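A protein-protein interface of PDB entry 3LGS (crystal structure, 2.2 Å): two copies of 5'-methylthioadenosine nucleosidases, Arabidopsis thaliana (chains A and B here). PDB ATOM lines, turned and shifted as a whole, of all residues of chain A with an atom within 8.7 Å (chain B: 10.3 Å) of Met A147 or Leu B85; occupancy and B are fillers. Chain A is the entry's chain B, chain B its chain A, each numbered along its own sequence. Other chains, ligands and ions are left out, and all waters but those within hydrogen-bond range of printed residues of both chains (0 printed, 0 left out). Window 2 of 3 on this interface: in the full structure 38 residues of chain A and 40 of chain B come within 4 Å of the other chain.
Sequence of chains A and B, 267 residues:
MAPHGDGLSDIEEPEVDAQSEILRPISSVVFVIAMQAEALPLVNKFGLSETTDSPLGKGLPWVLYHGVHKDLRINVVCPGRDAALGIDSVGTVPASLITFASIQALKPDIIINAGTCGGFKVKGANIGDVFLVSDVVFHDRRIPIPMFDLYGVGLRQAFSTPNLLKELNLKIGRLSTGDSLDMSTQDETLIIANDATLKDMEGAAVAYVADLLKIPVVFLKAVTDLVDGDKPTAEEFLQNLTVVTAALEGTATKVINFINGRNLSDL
O of Val B90 is in hydrogen-bond range of OH of Tyr A151.
The backbone NH (N) of Met A147 lies within hydrogen-bond range of the side-chain carboxylate (OD1) of Asp A149 (3.1 Å). The backbone carbonyl oxygen (O) of Ile A143 sits close to the backbone NH (N) of Asp A149, at 3.2 Å. The backbone NH (N) of Asp B82 sits at hydrogen-bond distance from the backbone carbonyl oxygen (O) of Ile B87, 2.7 Å away. O of Gly B80 lies within hydrogen-bond range of OG of Ser B89, 2.7 Å away. The backbone NH of Ala B84 sits close to the side-chain carboxylate of Asp B82 (3.4 Å).
Ile A143 touches Val B90. SD of Met A147 touches CG of Leu B85, 3.9 Å away. Met A147 touches Ile B87 (CE to CG2, 3.5 Å). Ile B87 touches Phe A148. CE1 of Phe A148 touches O of Asp B88, at 3.8 Å. Asp B82 touches Tyr A151. CB of Tyr A151 touches CD1 of Ile B87, 3.6 Å away. Tyr A151 touches Ser B89 (OH to C, 3.2 Å).
Printed residues of chain B within 4 Å of Ile A143: Val B90 (3.9 Å). No residue of chain B comes within 4 Å of Pro A146. Met A147 touches just these residues of chain B: Leu B85 (3.9 Å) and Ile B87 (3.5 Å). Of chain B, only Ile B87 and Asp B88 come within 4 Å of Phe A148. Asp A149 touches none of the printed residues of chain B. No residue of chain B comes within 4 Å of Leu A150. Of the printed residues of chain B, Tyr A151 touches Asp B82, Ile B87, Ser B89 and Val B90. Printed residues of chain A within 4 Å of Asp B82: Tyr A151. Ala B84 touches none of the printed residues of chain A. Of chain A, only Met A147 comes within 4 Å of Leu B85. Printed residues of chain A within 4 Å of Ile B87: Met A147, Phe A148 and Tyr A151. Of the printed residues of chain A, Asp B88 touches Phe A148. The nearest residue of chain A that does not touch Leu B85 is Leu A150 (6.1 Å).
Of the 12 printed residues of chain A, 4 touch a printed residue of chain B. Hydrophobic or aromatic side chains of chain A that line the printed part of chain B: Ile A143, Met A147, Phe A148 and Tyr A151. Along chain A the printed residues that touch a printed residue of chain B span positions 143 to 151. Of the 13 printed residues of chain B, 6 touch a printed residue of chain A. Printed residues of chain B that touch a printed residue of chain A: Asp B82, Leu B85, Ile B87, Asp B88, Ser B89 and Val B90. Hydrophobic or aromatic side chains of chain B within 4 Å of the printed part of chain A: Leu B85, Ile B87 and Val B90. Among the printed residues, 9 pairs touch across the chains. Among the printed residues, no Asp or Glu carboxylate lies within 4 Å of a Lys or Arg side-chain nitrogen of the other chain.
No position is printed for both chains. Of the 9 pairs that touch across the chains among the printed residues, none has its exchanged pair printed and touching as well.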
ATOM      1  N   ILE A 143       6.838  -1.530  10.875  1.00  0.00           N
ATOM      2  CA  ILE A 143       7.066  -0.515   9.859  1.00  0.00           C
ATOM      3  C   ILE A 143       6.430   0.796  10.337  1.00  0.00           C
ATOM      4  O   ILE A 143       5.217   1.017  10.135  1.00  0.00           O
ATOM      5  CB  ILE A 143       6.507  -0.936   8.480  1.00  0.00           C
ATOM      6  CG1 ILE A 143       6.921  -2.383   8.148  1.00  0.00           C
ATOM      7  CG2 ILE A 143       7.026   0.028   7.385  1.00  0.00           C
ATOM      8  CD1 ILE A 143       6.172  -3.011   6.978  1.00  0.00           C
ATOM      9  N   PRO A 144       7.246   1.679  10.954  1.00  0.00           N
ATOM     10  CA  PRO A 144       6.674   2.853  11.628  1.00  0.00           C
ATOM     11  C   PRO A 144       6.340   3.997  10.659  1.00  0.00           C
ATOM     12  O   PRO A 144       6.840   5.113  10.775  1.00  0.00           O
ATOM     13  CB  PRO A 144       7.748   3.222  12.651  1.00  0.00           C
ATOM     14  CG  PRO A 144       9.040   2.772  12.009  1.00  0.00           C
ATOM     15  CD  PRO A 144       8.720   1.661  11.036  1.00  0.00           C
ATOM     16  N   ILE A 145       5.502   3.677   9.680  1.00  0.00           N
ATOM     17  CA  ILE A 145       4.950   4.639   8.723  1.00  0.00           C
ATOM     18  C   ILE A 145       3.472   4.307   8.662  1.00  0.00           C
ATOM     19  O   ILE A 145       3.135   3.124   8.561  1.00  0.00           O
ATOM     20  CB  ILE A 145       5.530   4.442   7.312  1.00  0.00           C
ATOM     21  CG1 ILE A 145       7.068   4.507   7.315  1.00  0.00           C
ATOM     22  CG2 ILE A 145       4.966   5.479   6.353  1.00  0.00           C
ATOM     23  CD1 ILE A 145       7.720   4.050   6.002  1.00  0.00           C
ATOM     24  N   PRO A 146       2.588   5.329   8.729  1.00  0.00           N
ATOM     25  CA  PRO A 146       1.148   5.081   8.583  1.00  0.00           C
ATOM     26  C   PRO A 146       0.818   4.204   7.371  1.00  0.00           C
ATOM     27  O   PRO A 146       1.486   4.301   6.343  1.00  0.00           O
ATOM     28  CB  PRO A 146       0.563   6.494   8.411  1.00  0.00           C
ATOM     29  CG  PRO A 146       1.490   7.394   9.162  1.00  0.00           C
ATOM     30  CD  PRO A 146       2.875   6.756   9.018  1.00  0.00           C
ATOM     31  N   MET A 147      -0.193   3.346   7.523  1.00  0.00           N
ATOM     32  CA  MET A 147      -0.672   2.417   6.487  1.00  0.00           C
ATOM     33  C   MET A 147       0.229   1.180   6.435  1.00  0.00           C
ATOM     34  O   MET A 147      -0.253   0.041   6.560  1.00  0.00           O
ATOM     35  CB  MET A 147      -0.778   3.070   5.101  1.00  0.00           C
ATOM     36  CG  MET A 147      -1.552   4.426   5.049  1.00  0.00           C
ATOM     37  SD  MET A 147      -1.750   5.112   3.375  1.00  0.00           S
ATOM     38  CE  MET A 147      -0.060   5.445   2.879  1.00  0.00           C
ATOM     39  N   PHE A 148       1.524   1.408   6.255  1.00  0.00           N
ATOM     40  CA  PHE A 148       2.510   0.338   6.368  1.00  0.00           C
ATOM     41  C   PHE A 148       2.493  -0.331   7.740  1.00  0.00           C
ATOM     42  O   PHE A 148       2.615  -1.539   7.815  1.00  0.00           O
ATOM     43  CB  PHE A 148       3.917   0.845   6.069  1.00  0.00           C
ATOM     44  CG  PHE A 148       4.168   1.146   4.620  1.00  0.00           C
ATOM     45  CD1 PHE A 148       4.536   0.131   3.738  1.00  0.00           C
ATOM     46  CD2 PHE A 148       4.072   2.448   4.143  1.00  0.00           C
ATOM     47  CE1 PHE A 148       4.797   0.403   2.391  1.00  0.00           C
ATOM     48  CE2 PHE A 148       4.329   2.735   2.801  1.00  0.00           C
ATOM     49  CZ  PHE A 148       4.693   1.704   1.920  1.00  0.00           C
ATOM     50  N   ASP A 149       2.318   0.447   8.811  1.00  0.00           N
ATOM     51  CA  ASP A 149       2.244  -0.133  10.159  1.00  0.00           C
ATOM     52  C   ASP A 149       1.153  -1.200  10.262  1.00  0.00           C
ATOM     53  O   ASP A 149       1.409  -2.293  10.772  1.00  0.00           O
ATOM     54  CB  ASP A 149       2.175   0.918  11.297  1.00  0.00           C
ATOM     55  CG  ASP A 149       0.992   1.907  11.167  1.00  0.00           C
ATOM     56  OD1 ASP A 149       0.170   1.813  10.227  1.00  0.00           O
ATOM     57  OD2 ASP A 149       0.889   2.810  12.028  1.00  0.00           O
ATOM     58  N   LEU A 150      -0.038  -0.907   9.742  1.00  0.00           N
ATOM     59  CA  LEU A 150      -1.171  -1.848   9.832  1.00  0.00           C
ATOM     60  C   LEU A 150      -0.977  -3.070   8.933  1.00  0.00           C
ATOM     61  O   LEU A 150      -1.311  -4.205   9.305  1.00  0.00           O
ATOM     62  CB  LEU A 150      -2.498  -1.138   9.519  1.00  0.00           C
ATOM     63  CG  LEU A 150      -2.880   0.026  10.448  1.00  0.00           C
ATOM     64  CD1 LEU A 150      -4.226   0.621  10.039  1.00  0.00           C
ATOM     65  CD2 LEU A 150      -2.880  -0.357  11.939  1.00  0.00           C
ATOM     66  N   TYR A 151      -0.430  -2.812   7.748  1.00  0.00           N
ATOM     67  CA  TYR A 151      -0.037  -3.842   6.818  1.00  0.00           C
ATOM     68  C   TYR A 151       0.925  -4.833   7.485  1.00  0.00           C
ATOM     69  O   TYR A 151       0.737  -6.067   7.406  1.00  0.00           O
ATOM     70  CB  TYR A 151       0.614  -3.197   5.576  1.00  0.00           C
ATOM     71  CG  TYR A 151       1.327  -4.201   4.729  1.00  0.00           C
ATOM     72  CD1 TYR A 151       0.611  -5.058   3.894  1.00  0.00           C
ATOM     73  CD2 TYR A 151       2.722  -4.343   4.798  1.00  0.00           C
ATOM     74  CE1 TYR A 151       1.261  -6.001   3.111  1.00  0.00           C
ATOM     75  CE2 TYR A 151       3.376  -5.282   4.036  1.00  0.00           C
ATOM     76  CZ  TYR A 151       2.635  -6.111   3.199  1.00  0.00           C
ATOM     77  OH  TYR A 151       3.248  -7.052   2.446  1.00  0.00           O
ATOM     78  N   GLY A 152       1.949  -4.294   8.141  1.00  0.00           N
ATOM     79  CA  GLY A 152       2.940  -5.108   8.845  1.00  0.00           C
ATOM     80  C   GLY A 152       2.307  -6.032   9.867  1.00  0.00           C
ATOM     81  O   GLY A 152       2.563  -7.243   9.874  1.00  0.00           O
ATOM     82  N   VAL A 153       1.472  -5.445  10.723  1.00  0.00           N
ATOM     83  CA  VAL A 153       0.746  -6.168  11.755  1.00  0.00           C
ATOM     84  C   VAL A 153      -0.127  -7.231  11.094  1.00  0.00           C
ATOM     85  O   VAL A 153      -0.224  -8.356  11.597  1.00  0.00           O
ATOM     86  CB  VAL A 153      -0.094  -5.182  12.646  1.00  0.00           C
ATOM     87  CG1 VAL A 153      -1.049  -5.921  13.622  1.00  0.00           C
ATOM     88  CG2 VAL A 153       0.840  -4.199  13.411  1.00  0.00           C
ATOM     89  N   GLY A 154      -0.734  -6.863   9.959  1.00  0.00           N
ATOM     90  CA  GLY A 154      -1.528  -7.760   9.125  1.00  0.00           C
ATOM     91  C   GLY A 154      -2.645  -8.481   9.849  1.00  0.00           C
ATOM     92  O   GLY A 154      -2.742  -9.715   9.774  1.00  0.00           O
ATOM     93  N   MET B  35       8.729  -2.390  -4.427  1.00  0.00           N
ATOM     94  CA  MET B  35       7.885  -1.190  -4.586  1.00  0.00           C
ATOM     95  C   MET B  35       7.644  -0.797  -6.049  1.00  0.00           C
ATOM     96  O   MET B  35       8.585  -0.694  -6.822  1.00  0.00           O
ATOM     97  CB  MET B  35       8.503  -0.017  -3.832  1.00  0.00           C
ATOM     98  CG  MET B  35       8.797  -0.328  -2.360  1.00  0.00           C
ATOM     99  SD  MET B  35       9.483   1.088  -1.511  1.00  0.00           S
ATOM    100  CE  MET B  35       8.025   1.970  -1.050  1.00  0.00           C
ATOM    101  N   GLY B  80       2.906  -6.049  -5.665  1.00  0.00           N
ATOM    102  CA  GLY B  80       1.653  -5.353  -5.850  1.00  0.00           C
ATOM    103  C   GLY B  80       1.244  -4.488  -4.690  1.00  0.00           C
ATOM    104  O   GLY B  80       1.752  -4.607  -3.560  1.00  0.00           O
ATOM    105  N   ARG B  81       0.299  -3.612  -4.985  1.00  0.00           N
ATOM    106  CA  ARG B  81      -0.247  -2.705  -4.005  1.00  0.00           C
ATOM    107  C   ARG B  81      -1.288  -3.453  -3.207  1.00  0.00           C
ATOM    108  O   ARG B  81      -2.116  -4.155  -3.767  1.00  0.00           O
ATOM    109  CB  ARG B  81      -0.836  -1.479  -4.711  1.00  0.00           C
ATOM    110  CG  ARG B  81       0.252  -0.583  -5.343  1.00  0.00           C
ATOM    111  CD  ARG B  81      -0.151  -0.049  -6.725  1.00  0.00           C
ATOM    112  NE  ARG B  81       0.877   0.847  -7.266  1.00  0.00           N
ATOM    113  CZ  ARG B  81       0.694   1.697  -8.281  1.00  0.00           C
ATOM    114  NH1 ARG B  81      -0.496   1.774  -8.893  1.00  0.00           N
ATOM    115  NH2 ARG B  81       1.704   2.472  -8.684  1.00  0.00           N
ATOM    116  N   ASP B  82      -1.209  -3.310  -1.890  1.00  0.00           N
ATOM    117  CA  ASP B  82      -2.098  -3.947  -0.930  1.00  0.00           C
ATOM    118  C   ASP B  82      -3.557  -3.495  -1.098  1.00  0.00           C
ATOM    119  O   ASP B  82      -3.822  -2.370  -1.530  1.00  0.00           O
ATOM    120  CB  ASP B  82      -1.593  -3.638   0.487  1.00  0.00           C
ATOM    121  CG  ASP B  82      -2.290  -4.455   1.554  1.00  0.00           C
ATOM    122  OD1 ASP B  82      -2.052  -5.686   1.621  1.00  0.00           O
ATOM    123  OD2 ASP B  82      -3.085  -3.864   2.313  1.00  0.00           O
ATOM    124  N   ALA B  83      -4.493  -4.382  -0.748  1.00  0.00           N
ATOM    125  CA  ALA B  83      -5.920  -4.163  -1.015  1.00  0.00           C
ATOM    126  C   ALA B  83      -6.533  -3.014  -0.218  1.00  0.00           C
ATOM    127  O   ALA B  83      -7.436  -2.358  -0.705  1.00  0.00           O
ATOM    128  CB  ALA B  83      -6.728  -5.480  -0.808  1.00  0.00           C
ATOM    129  N   ALA B  84      -6.027  -2.762   0.988  1.00  0.00           N
ATOM    130  CA  ALA B  84      -6.604  -1.771   1.886  1.00  0.00           C
ATOM    131  C   ALA B  84      -6.379  -0.311   1.441  1.00  0.00           C
ATOM    132  O   ALA B  84      -7.352   0.420   1.160  1.00  0.00           O
ATOM    133  CB  ALA B  84      -6.096  -1.980   3.293  1.00  0.00           C
ATOM    134  N   LEU B  85      -5.108   0.100   1.376  1.00  0.00           N
ATOM    135  CA  LEU B  85      -4.734   1.497   1.145  1.00  0.00           C
ATOM    136  C   LEU B  85      -3.909   1.743  -0.118  1.00  0.00           C
ATOM    137  O   LEU B  85      -3.714   2.909  -0.547  1.00  0.00           O
ATOM    138  CB  LEU B  85      -3.956   2.014   2.340  1.00  0.00           C
ATOM    139  CG  LEU B  85      -4.788   2.679   3.432  1.00  0.00           C
ATOM    140  CD1 LEU B  85      -5.674   3.806   2.870  1.00  0.00           C
ATOM    141  CD2 LEU B  85      -5.612   1.659   4.183  1.00  0.00           C
ATOM    142  N   GLY B  86      -3.403   0.663  -0.704  1.00  0.00           N
ATOM    143  CA  GLY B  86      -2.677   0.768  -1.956  1.00  0.00           C
ATOM    144  C   GLY B  86      -1.172   0.825  -1.795  1.00  0.00           C
ATOM    145  O   GLY B  86      -0.461   1.100  -2.766  1.00  0.00           O
ATOM    146  N   ILE B  87      -0.679   0.558  -0.586  1.00  0.00           N
ATOM    147  CA  ILE B  87       0.751   0.574  -0.367  1.00  0.00           C
ATOM    148  C   ILE B  87       1.425  -0.710  -0.866  1.00  0.00           C
ATOM    149  O   ILE B  87       0.803  -1.770  -0.896  1.00  0.00           O
ATOM    150  CB  ILE B  87       1.134   0.947   1.100  1.00  0.00           C
ATOM    151  CG1 ILE B  87       0.329   0.142   2.123  1.00  0.00           C
ATOM    152  CG2 ILE B  87       0.891   2.417   1.328  1.00  0.00           C
ATOM    153  CD1 ILE B  87       1.119  -0.965   2.785  1.00  0.00           C
ATOM    154  N   ASP B  88       2.684  -0.589  -1.286  1.00  0.00           N
ATOM    155  CA  ASP B  88       3.485  -1.738  -1.717  1.00  0.00           C
ATOM    156  C   ASP B  88       3.467  -2.864  -0.681  1.00  0.00           C
ATOM    157  O   ASP B  88       3.579  -2.614   0.515  1.00  0.00           O
ATOM    158  CB  ASP B  88       4.925  -1.296  -1.995  1.00  0.00           C
ATOM    159  CG  ASP B  88       5.022  -0.347  -3.186  1.00  0.00           C
ATOM    160  OD1 ASP B  88       4.604  -0.734  -4.296  1.00  0.00           O
ATOM    161  OD2 ASP B  88       5.516   0.780  -3.000  1.00  0.00           O
ATOM    162  N   SER B  89       3.289  -4.098  -1.140  1.00  0.00           N
ATOM    163  CA  SER B  89       3.274  -5.241  -0.233  1.00  0.00           C
ATOM    164  C   SER B  89       4.718  -5.651   0.018  1.00  0.00           C
ATOM    165  O   SER B  89       5.213  -6.598  -0.568  1.00  0.00           O
ATOM    166  CB  SER B  89       2.455  -6.407  -0.807  1.00  0.00           C
ATOM    167  OG  SER B  89       1.175  -5.978  -1.254  1.00  0.00           O
ATOM    168  N   VAL B  90       5.383  -4.906   0.884  1.00  0.00           N
ATOM    169  CA  VAL B  90       6.791  -5.134   1.229  1.00  0.00           C
ATOM    170  C   VAL B  90       6.953  -6.327   2.184  1.00  0.00           C
ATOM    171  O   VAL B  90       5.964  -6.875   2.699  1.00  0.00           O
ATOM    172  CB  VAL B  90       7.432  -3.839   1.846  1.00  0.00           C
ATOM    173  CG1 VAL B  90       7.450  -2.653   0.804  1.00  0.00           C
ATOM    174  CG2 VAL B  90       6.708  -3.446   3.120  1.00  0.00           C
ATOM    175  N   LEU B 238      11.939   7.975   3.376  1.00  0.00           N
ATOM    176  CA  LEU B 238      10.909   8.623   2.559  1.00  0.00           C
ATOM    177  C   LEU B 238      11.460   9.869   1.848  1.00  0.00           C
ATOM    178  O   LEU B 238      11.133  10.137   0.680  1.00  0.00           O
ATOM    179  CB  LEU B 238       9.676   8.967   3.408  1.00  0.00           C
ATOM    180  CG  LEU B 238       8.885   7.791   3.996  1.00  0.00           C
ATOM    181  CD1 LEU B 238       7.878   8.271   5.051  1.00  0.00           C
ATOM    182  CD2 LEU B 238       8.190   6.974   2.908  1.00  0.00           C
